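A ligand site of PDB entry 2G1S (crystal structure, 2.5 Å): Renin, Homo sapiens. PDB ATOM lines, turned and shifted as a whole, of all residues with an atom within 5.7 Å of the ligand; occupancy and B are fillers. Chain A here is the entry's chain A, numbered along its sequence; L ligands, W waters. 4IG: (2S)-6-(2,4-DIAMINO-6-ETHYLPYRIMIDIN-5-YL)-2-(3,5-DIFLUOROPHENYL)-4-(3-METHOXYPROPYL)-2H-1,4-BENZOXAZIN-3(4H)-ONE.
Merely in contact with the ligand: Leu 114, Ser 223, Thr 220, Gly 221, Thr 11, Gly 33, Tyr 76, Val 29, Pro 111, Val 120, Phe 117, Tyr 155 and Phe 112. Hydrophobic or aromatic side chains that line the ligand: Tyr 13, Val 29, Tyr 76, Pro 111, Phe 112, Leu 114, Phe 117 and Val 120. Within 4 Å of the ligand: Thr 11, Gln 12, Tyr 13, Val 29, Asp 31, Gly 33, Tyr 76, Ser 77, Thr 78, Pro 111, Phe 112, Leu 114, Phe 117, Val 120, Tyr 155, Asp 219, Thr 220, Gly 221 and Ser 223.
The side-chain hydroxyl of Ser 34 sits at hydrogen-bond distance from the side-chain carboxylate of Asp 31. The side-chain carboxylate of Asp 31 sits close to the backbone NH of Gly 221, at 3.4 Å. The backbone carbonyl oxygen (O) of Thr 220 is in hydrogen-bond range of the side-chain hydroxyl (OH) of Tyr 155 (2.8 Å). The side-chain hydroxyl of Thr 32 lies within hydrogen-bond range of the backbone NH of Thr 220 (2.7 Å). The backbone carbonyl oxygen (O) of Ser 223 lies close to the backbone NH (N) of Ala 310 (3.4 Å). The side-chain hydroxyl of Ser 223 is in hydrogen-bond range of the backbone carbonyl oxygen of Thr 11. OD2 of Asp 219 is in hydrogen-bond range of N of Gly 221 (2.8 Å). OD2 of Asp 219 lies within hydrogen-bond range of N of Gly 33 (3.2 Å).
The side-chain hydroxyl (OG1) of Thr 78 is in hydrogen-bond range of a nitrogen (N3) of the ligand (3.3 Å). The side-chain hydroxyl (OG) of Ser 77 is in hydrogen-bond range of a nitrogen (N3) of the ligand (3.1 Å). OD1 of Asp 219 lies within hydrogen-bond range of N4 of the ligand (2.7 Å). The backbone NH (N) of Tyr 13 sits at hydrogen-bond distance from an oxygen (O1) of the ligand. OD1 of Asp 31 lies within hydrogen-bond range of N2 of the ligand, at 2.6 Å. The side-chain amide nitrogen of Gln 12 lies close to an oxygen (O4) of the ligand (3.2 Å).
Water W5 lies within hydrogen-bond range of the backbone NH of Ser 77 (2.9 Å) and a nitrogen (N1) of the ligand (2.9 Å). Water W2 lies within hydrogen-bond range of NE2 of Gln 12 (2.8 Å), O4 of the ligand (3.0 Å) and OG1 of Thr 11 (3.1 Å). Water W4 lies within hydrogen-bond range of the backbone carbonyl oxygen of Gly 33 (2.8 Å) and a nitrogen (N4) of the ligand (3.1 Å).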
ATOM      1  N   THR A  11      -5.300  24.437 -16.637  1.00  0.00           N
ATOM      2  CA  THR A  11      -4.832  25.302 -17.703  1.00  0.00           C
ATOM      3  C   THR A  11      -4.360  24.512 -18.920  1.00  0.00           C
ATOM      4  O   THR A  11      -4.189  25.078 -19.994  1.00  0.00           O
ATOM      5  CB  THR A  11      -3.686  26.215 -17.240  1.00  0.00           C
ATOM      6  OG1 THR A  11      -2.516  25.416 -16.995  1.00  0.00           O
ATOM      7  CG2 THR A  11      -4.068  26.961 -15.990  1.00  0.00           C
ATOM      8  N   GLN A  12      -4.133  23.220 -18.746  1.00  0.00           N
ATOM      9  CA  GLN A  12      -3.672  22.379 -19.839  1.00  0.00           C
ATOM     10  C   GLN A  12      -4.486  21.085 -19.935  1.00  0.00           C
ATOM     11  O   GLN A  12      -4.607  20.337 -18.967  1.00  0.00           O
ATOM     12  CB  GLN A  12      -2.192  22.048 -19.648  1.00  0.00           C
ATOM     13  CG  GLN A  12      -1.270  23.255 -19.741  1.00  0.00           C
ATOM     14  CD  GLN A  12       0.183  22.912 -19.505  1.00  0.00           C
ATOM     15  OE1 GLN A  12       0.712  21.949 -20.067  1.00  0.00           O
ATOM     16  NE2 GLN A  12       0.860  23.703 -18.663  1.00  0.00           N
ATOM     17  N   TYR A  13      -5.065  20.844 -21.111  1.00  0.00           N
ATOM     18  CA  TYR A  13      -5.846  19.636 -21.367  1.00  0.00           C
ATOM     19  C   TYR A  13      -5.233  18.932 -22.580  1.00  0.00           C
ATOM     20  O   TYR A  13      -5.097  19.526 -23.653  1.00  0.00           O
ATOM     21  CB  TYR A  13      -7.324  19.987 -21.642  1.00  0.00           C
ATOM     22  CG  TYR A  13      -8.071  20.545 -20.441  1.00  0.00           C
ATOM     23  CD1 TYR A  13      -7.871  21.852 -20.004  1.00  0.00           C
ATOM     24  CD2 TYR A  13      -8.970  19.755 -19.726  1.00  0.00           C
ATOM     25  CE1 TYR A  13      -8.541  22.352 -18.899  1.00  0.00           C
ATOM     26  CE2 TYR A  13      -9.640  20.254 -18.621  1.00  0.00           C
ATOM     27  CZ  TYR A  13      -9.425  21.553 -18.208  1.00  0.00           C
ATOM     28  OH  TYR A  13     -10.065  22.054 -17.114  1.00  0.00           O
ATOM     29  N   VAL A  29      -2.412  18.708 -27.255  1.00  0.00           N
ATOM     30  CA  VAL A  29      -3.620  19.472 -26.969  1.00  0.00           C
ATOM     31  C   VAL A  29      -4.455  19.523 -28.237  1.00  0.00           C
ATOM     32  O   VAL A  29      -3.917  19.760 -29.330  1.00  0.00           O
ATOM     33  CB  VAL A  29      -3.291  20.919 -26.540  1.00  0.00           C
ATOM     34  CG1 VAL A  29      -4.567  21.748 -26.510  1.00  0.00           C
ATOM     35  CG2 VAL A  29      -2.635  20.934 -25.177  1.00  0.00           C
ATOM     36  N   ASP A  31      -6.587  21.473 -30.303  1.00  0.00           N
ATOM     37  CA  ASP A  31      -6.778  22.912 -30.488  1.00  0.00           C
ATOM     38  C   ASP A  31      -7.684  23.430 -31.609  1.00  0.00           C
ATOM     39  O   ASP A  31      -7.250  23.505 -32.764  1.00  0.00           O
ATOM     40  CB  ASP A  31      -5.377  23.502 -30.639  1.00  0.00           C
ATOM     41  CG  ASP A  31      -5.364  24.985 -30.832  1.00  0.00           C
ATOM     42  OD1 ASP A  31      -4.331  25.483 -31.310  1.00  0.00           O
ATOM     43  OD2 ASP A  31      -6.365  25.667 -30.503  1.00  0.00           O
ATOM     44  N   THR A  32      -8.902  23.836 -31.267  1.00  0.00           N
ATOM     45  CA  THR A  32      -9.824  24.391 -32.268  1.00  0.00           C
ATOM     46  C   THR A  32      -9.305  25.742 -32.750  1.00  0.00           C
ATOM     47  O   THR A  32      -9.803  26.279 -33.724  1.00  0.00           O
ATOM     48  CB  THR A  32     -11.252  24.649 -31.698  1.00  0.00           C
ATOM     49  OG1 THR A  32     -11.172  25.550 -30.585  1.00  0.00           O
ATOM     50  CG2 THR A  32     -11.916  23.340 -31.271  1.00  0.00           C
ATOM     51  N   GLY A  33      -8.300  26.266 -32.046  1.00  0.00           N
ATOM     52  CA  GLY A  33      -7.724  27.552 -32.413  1.00  0.00           C
ATOM     53  C   GLY A  33      -6.601  27.518 -33.442  1.00  0.00           C
ATOM     54  O   GLY A  33      -6.092  28.572 -33.812  1.00  0.00           O
ATOM     55  N   SER A  34      -6.201  26.333 -33.889  1.00  0.00           N
ATOM     56  CA  SER A  34      -5.146  26.202 -34.897  1.00  0.00           C
ATOM     57  C   SER A  34      -5.546  25.090 -35.883  1.00  0.00           C
ATOM     58  O   SER A  34      -6.554  24.413 -35.678  1.00  0.00           O
ATOM     59  CB  SER A  34      -3.789  25.924 -34.233  1.00  0.00           C
ATOM     60  OG  SER A  34      -3.727  24.626 -33.657  1.00  0.00           O
ATOM     61  N   TYR A  76       1.457  30.955 -32.256  1.00  0.00           N
ATOM     62  CA  TYR A  76       0.320  30.968 -31.364  1.00  0.00           C
ATOM     63  C   TYR A  76       0.394  32.283 -30.615  1.00  0.00           C
ATOM     64  O   TYR A  76       1.410  32.973 -30.647  1.00  0.00           O
ATOM     65  CB  TYR A  76       0.371  29.778 -30.395  1.00  0.00           C
ATOM     66  CG  TYR A  76       0.405  28.435 -31.076  1.00  0.00           C
ATOM     67  CD1 TYR A  76       1.587  27.736 -31.209  1.00  0.00           C
ATOM     68  CD2 TYR A  76      -0.748  27.871 -31.622  1.00  0.00           C
ATOM     69  CE1 TYR A  76       1.640  26.517 -31.864  1.00  0.00           C
ATOM     70  CE2 TYR A  76      -0.708  26.648 -32.283  1.00  0.00           C
ATOM     71  CZ  TYR A  76       0.492  25.973 -32.401  1.00  0.00           C
ATOM     72  OH  TYR A  76       0.567  24.780 -33.072  1.00  0.00           O
ATOM     73  N   SER A  77      -0.688  32.641 -29.930  1.00  0.00           N
ATOM     74  CA  SER A  77      -0.723  33.886 -29.195  1.00  0.00           C
ATOM     75  C   SER A  77       0.318  33.941 -28.065  1.00  0.00           C
ATOM     76  O   SER A  77       0.701  35.021 -27.619  1.00  0.00           O
ATOM     77  CB  SER A  77      -2.126  34.102 -28.612  1.00  0.00           C
ATOM     78  OG  SER A  77      -2.489  33.017 -27.784  1.00  0.00           O
ATOM     79  N   THR A  78       0.782  32.793 -27.605  1.00  0.00           N
ATOM     80  CA  THR A  78       1.730  32.811 -26.495  1.00  0.00           C
ATOM     81  C   THR A  78       3.087  32.167 -26.767  1.00  0.00           C
ATOM     82  O   THR A  78       3.885  31.992 -25.852  1.00  0.00           O
ATOM     83  CB  THR A  78       1.102  32.153 -25.256  1.00  0.00           C
ATOM     84  OG1 THR A  78       0.620  30.846 -25.592  1.00  0.00           O
ATOM     85  CG2 THR A  78      -0.046  32.996 -24.747  1.00  0.00           C
ATOM     86  N   GLY A  79       3.354  31.836 -28.030  1.00  0.00           N
ATOM     87  CA  GLY A  79       4.624  31.222 -28.366  1.00  0.00           C
ATOM     88  C   GLY A  79       4.677  30.725 -29.797  1.00  0.00           C
ATOM     89  O   GLY A  79       3.637  30.552 -30.445  1.00  0.00           O
ATOM     90  N   PRO A 111       7.357  29.491 -23.823  1.00  0.00           N
ATOM     91  CA  PRO A 111       6.695  28.808 -22.711  1.00  0.00           C
ATOM     92  C   PRO A 111       6.750  27.280 -22.690  1.00  0.00           C
ATOM     93  O   PRO A 111       6.237  26.660 -21.756  1.00  0.00           O
ATOM     94  CB  PRO A 111       5.245  29.233 -22.896  1.00  0.00           C
ATOM     95  CG  PRO A 111       5.105  29.037 -24.419  1.00  0.00           C
ATOM     96  CD  PRO A 111       6.418  29.683 -24.947  1.00  0.00           C
ATOM     97  N   PHE A 112       7.348  26.650 -23.692  1.00  0.00           N
ATOM     98  CA  PHE A 112       7.296  25.200 -23.727  1.00  0.00           C
ATOM     99  C   PHE A 112       7.874  24.374 -22.609  1.00  0.00           C
ATOM    100  O   PHE A 112       7.460  23.229 -22.434  1.00  0.00           O
ATOM    101  CB  PHE A 112       7.733  24.719 -25.093  1.00  0.00           C
ATOM    102  CG  PHE A 112       6.865  25.249 -26.183  1.00  0.00           C
ATOM    103  CD1 PHE A 112       7.274  26.320 -26.961  1.00  0.00           C
ATOM    104  CD2 PHE A 112       5.576  24.755 -26.359  1.00  0.00           C
ATOM    105  CE1 PHE A 112       6.410  26.892 -27.874  1.00  0.00           C
ATOM    106  CE2 PHE A 112       4.713  25.327 -27.272  1.00  0.00           C
ATOM    107  CZ  PHE A 112       5.123  26.390 -28.030  1.00  0.00           C
ATOM    108  N   LEU A 114       7.159  24.926 -19.793  1.00  0.00           N
ATOM    109  CA  LEU A 114       6.003  24.899 -18.903  1.00  0.00           C
ATOM    110  C   LEU A 114       4.867  24.089 -19.492  1.00  0.00           C
ATOM    111  O   LEU A 114       3.778  24.023 -18.924  1.00  0.00           O
ATOM    112  CB  LEU A 114       5.520  26.317 -18.620  1.00  0.00           C
ATOM    113  CG  LEU A 114       6.577  27.245 -18.022  1.00  0.00           C
ATOM    114  CD1 LEU A 114       5.993  28.630 -17.881  1.00  0.00           C
ATOM    115  CD2 LEU A 114       7.051  26.703 -16.666  1.00  0.00           C
ATOM    116  N   ALA A 115       5.096  23.483 -20.650  1.00  0.00           N
ATOM    117  CA  ALA A 115       4.074  22.668 -21.298  1.00  0.00           C
ATOM    118  C   ALA A 115       4.138  21.230 -20.795  1.00  0.00           C
ATOM    119  O   ALA A 115       5.195  20.592 -20.818  1.00  0.00           O
ATOM    120  CB  ALA A 115       4.268  22.683 -22.793  1.00  0.00           C
ATOM    121  N   GLU A 116       2.998  20.727 -20.332  1.00  0.00           N
ATOM    122  CA  GLU A 116       2.936  19.355 -19.869  1.00  0.00           C
ATOM    123  C   GLU A 116       2.840  18.483 -21.120  1.00  0.00           C
ATOM    124  O   GLU A 116       3.317  17.358 -21.148  1.00  0.00           O
ATOM    125  CB  GLU A 116       1.710  19.141 -18.990  1.00  0.00           C
ATOM    126  CG  GLU A 116       2.031  18.899 -17.538  1.00  0.00           C
ATOM    127  CD  GLU A 116       2.879  17.649 -17.342  1.00  0.00           C
ATOM    128  OE1 GLU A 116       2.419  16.568 -17.749  1.00  0.00           O
ATOM    129  OE2 GLU A 116       3.987  17.766 -16.788  1.00  0.00           O
ATOM    130  N   PHE A 117       2.210  19.031 -22.154  1.00  0.00           N
ATOM    131  CA  PHE A 117       2.031  18.322 -23.419  1.00  0.00           C
ATOM    132  C   PHE A 117       3.286  18.414 -24.287  1.00  0.00           C
ATOM    133  O   PHE A 117       4.174  19.223 -24.030  1.00  0.00           O
ATOM    134  CB  PHE A 117       0.860  18.912 -24.211  1.00  0.00           C
ATOM    135  CG  PHE A 117       0.982  20.387 -24.484  1.00  0.00           C
ATOM    136  CD1 PHE A 117       0.467  21.321 -23.597  1.00  0.00           C
ATOM    137  CD2 PHE A 117       1.605  20.843 -25.636  1.00  0.00           C
ATOM    138  CE1 PHE A 117       0.561  22.684 -23.849  1.00  0.00           C
ATOM    139  CE2 PHE A 117       1.706  22.205 -25.904  1.00  0.00           C
ATOM    140  CZ  PHE A 117       1.190  23.132 -25.011  1.00  0.00           C
ATOM    141  N   VAL A 120       0.733  19.636 -30.623  1.00  0.00           N
ATOM    142  CA  VAL A 120      -0.613  20.118 -30.872  1.00  0.00           C
ATOM    143  C   VAL A 120      -1.315  19.461 -32.055  1.00  0.00           C
ATOM    144  O   VAL A 120      -0.706  19.178 -33.092  1.00  0.00           O
ATOM    145  CB  VAL A 120      -0.588  21.662 -31.132  1.00  0.00           C
ATOM    146  CG1 VAL A 120      -2.012  22.203 -31.299  1.00  0.00           C
ATOM    147  CG2 VAL A 120       0.148  22.374 -30.005  1.00  0.00           C
ATOM    148  N   TYR A 155     -14.294  19.564 -20.795  1.00  0.00           N
ATOM    149  CA  TYR A 155     -13.144  19.880 -19.953  1.00  0.00           C
ATOM    150  C   TYR A 155     -13.639  19.896 -18.507  1.00  0.00           C
ATOM    151  O   TYR A 155     -14.356  20.816 -18.104  1.00  0.00           O
ATOM    152  CB  TYR A 155     -12.566  21.250 -20.283  1.00  0.00           C
ATOM    153  CG  TYR A 155     -11.640  21.283 -21.465  1.00  0.00           C
ATOM    154  CD1 TYR A 155     -11.180  22.495 -21.961  1.00  0.00           C
ATOM    155  CD2 TYR A 155     -11.232  20.118 -22.090  1.00  0.00           C
ATOM    156  CE1 TYR A 155     -10.351  22.549 -23.063  1.00  0.00           C
ATOM    157  CE2 TYR A 155     -10.405  20.166 -23.199  1.00  0.00           C
ATOM    158  CZ  TYR A 155      -9.970  21.396 -23.676  1.00  0.00           C
ATOM    159  OH  TYR A 155      -9.158  21.469 -24.788  1.00  0.00           O
ATOM    160  N   ASP A 219     -11.973  28.710 -28.623  1.00  0.00           N
ATOM    161  CA  ASP A 219     -10.661  28.095 -28.692  1.00  0.00           C
ATOM    162  C   ASP A 219     -10.315  27.059 -27.609  1.00  0.00           C
ATOM    163  O   ASP A 219      -9.968  27.410 -26.476  1.00  0.00           O
ATOM    164  CB  ASP A 219      -9.662  29.241 -28.679  1.00  0.00           C
ATOM    165  CG  ASP A 219      -8.268  28.825 -29.003  1.00  0.00           C
ATOM    166  OD1 ASP A 219      -7.420  29.732 -29.133  1.00  0.00           O
ATOM    167  OD2 ASP A 219      -8.010  27.600 -29.120  1.00  0.00           O
ATOM    168  N   THR A 220     -10.385  25.777 -27.975  1.00  0.00           N
ATOM    169  CA  THR A 220     -10.069  24.702 -27.036  1.00  0.00           C
ATOM    170  C   THR A 220      -8.583  24.613 -26.713  1.00  0.00           C
ATOM    171  O   THR A 220      -8.176  23.876 -25.813  1.00  0.00           O
ATOM    172  CB  THR A 220     -10.524  23.326 -27.576  1.00  0.00           C
ATOM    173  OG1 THR A 220      -9.813  23.014 -28.781  1.00  0.00           O
ATOM    174  CG2 THR A 220     -12.023  23.336 -27.885  1.00  0.00           C
ATOM    175  N   GLY A 221      -7.765  25.371 -27.443  1.00  0.00           N
ATOM    176  CA  GLY A 221      -6.331  25.351 -27.212  1.00  0.00           C
ATOM    177  C   GLY A 221      -5.870  26.489 -26.333  1.00  0.00           C
ATOM    178  O   GLY A 221      -4.659  26.653 -26.103  1.00  0.00           O
ATOM    179  N   ALA A 222      -6.813  27.274 -25.828  1.00  0.00           N
ATOM    180  CA  ALA A 222      -6.518  28.410 -24.948  1.00  0.00           C
ATOM    181  C   ALA A 222      -6.944  28.100 -23.511  1.00  0.00           C
ATOM    182  O   ALA A 222      -8.044  27.606 -23.268  1.00  0.00           O
ATOM    183  CB  ALA A 222      -7.241  29.636 -25.444  1.00  0.00           C
ATOM    184  N   SER A 223      -6.078  28.401 -22.554  1.00  0.00           N
ATOM    185  CA  SER A 223      -6.390  28.121 -21.151  1.00  0.00           C
ATOM    186  C   SER A 223      -7.507  28.990 -20.607  1.00  0.00           C
ATOM    187  O   SER A 223      -8.387  28.523 -19.909  1.00  0.00           O
ATOM    188  CB  SER A 223      -5.146  28.306 -20.271  1.00  0.00           C
ATOM    189  OG  SER A 223      -4.051  27.529 -20.737  1.00  0.00           O
ATOM    190  N   ALA A 310     -10.617  27.312 -22.139  1.00  0.00           N
ATOM    191  CA  ALA A 310     -10.942  26.319 -21.120  1.00  0.00           C
ATOM    192  C   ALA A 310     -11.806  26.856 -19.985  1.00  0.00           C
ATOM    193  O   ALA A 310     -12.595  26.104 -19.402  1.00  0.00           O
ATOM    194  CB  ALA A 310      -9.665  25.719 -20.566  1.00  0.00           C
HETATM  195  C1  4IG L   1      -2.574  28.989 -27.843  1.00  0.00           C
HETATM  196  N1  4IG L   1      -3.692  29.230 -28.579  1.00  0.00           N
HETATM  197  C2  4IG L   1      -4.112  28.213 -29.343  1.00  0.00           C
HETATM  198  N2  4IG L   1      -3.514  27.024 -29.437  1.00  0.00           N
HETATM  199  C3  4IG L   1      -2.402  26.755 -28.703  1.00  0.00           C
HETATM  200  C4  4IG L   1      -1.886  27.743 -27.811  1.00  0.00           C
HETATM  201  N3  4IG L   1      -2.153  30.022 -27.091  1.00  0.00           N
HETATM  202  N4  4IG L   1      -5.220  28.386 -30.067  1.00  0.00           N
HETATM  203  C5  4IG L   1      -1.780  25.380 -28.877  1.00  0.00           C
HETATM  204  C6  4IG L   1      -2.539  24.281 -28.127  1.00  0.00           C
HETATM  205  C7  4IG L   1       0.561  27.601 -27.069  1.00  0.00           C
HETATM  206  C8  4IG L   1       1.508  27.307 -26.036  1.00  0.00           C
HETATM  207  C9  4IG L   1       1.064  26.876 -24.761  1.00  0.00           C
HETATM  208  C10 4IG L   1      -0.356  26.738 -24.508  1.00  0.00           C
HETATM  209  C11 4IG L   1      -1.241  27.043 -25.555  1.00  0.00           C
HETATM  210  C12 4IG L   1      -0.820  27.463 -26.828  1.00  0.00           C
HETATM  211  O3  4IG L   1       2.022  26.595 -23.742  1.00  0.00           O
HETATM  212  C14 4IG L   1       1.388  26.886 -22.478  1.00  0.00           C
HETATM  213  C15 4IG L   1       0.119  26.068 -22.183  1.00  0.00           C
HETATM  214  N5  4IG L   1      -0.796  26.312 -23.211  1.00  0.00           N
HETATM  215  C16 4IG L   1      -2.248  26.144 -22.856  1.00  0.00           C
HETATM  216  C17 4IG L   1      -2.804  24.764 -23.176  1.00  0.00           C
HETATM  217  C18 4IG L   1      -4.327  24.813 -23.362  1.00  0.00           C
HETATM  218  O1  4IG L   1      -4.827  23.496 -23.259  1.00  0.00           O
HETATM  219  C19 4IG L   1      -6.217  23.355 -23.412  1.00  0.00           C
HETATM  220  O4  4IG L   1      -0.034  25.397 -21.187  1.00  0.00           O
HETATM  221  C20 4IG L   1       2.569  28.993 -19.494  1.00  0.00           C
HETATM  222  C21 4IG L   1       2.346  27.827 -20.265  1.00  0.00           C
HETATM  223  C22 4IG L   1       1.884  27.986 -21.593  1.00  0.00           C
HETATM  224  C23 4IG L   1       1.686  29.287 -22.115  1.00  0.00           C
HETATM  225  C24 4IG L   1       1.922  30.406 -21.336  1.00  0.00           C
HETATM  226  C25 4IG L   1       2.365  30.302 -20.007  1.00  0.00           C
HETATM  227  F2  4IG L   1       2.996  28.868 -18.238  1.00  0.00           F
HETATM  228  F1  4IG L   1       1.696  31.593 -21.902  1.00  0.00           F
HETATM  229  O   HOH W   1      -1.225  29.766 -23.425  1.00  0.00           O
HETATM  230  O   HOH W   2       0.120  26.426 -18.356  1.00  0.00           O
HETATM  231  O   HOH W   3       0.093  34.403 -20.624  1.00  0.00           O
HETATM  232  O   HOH W   4      -3.819  29.672 -32.568  1.00  0.00           O
HETATM  233  O   HOH W   5      -3.161  31.304 -30.506  1.00  0.00           O
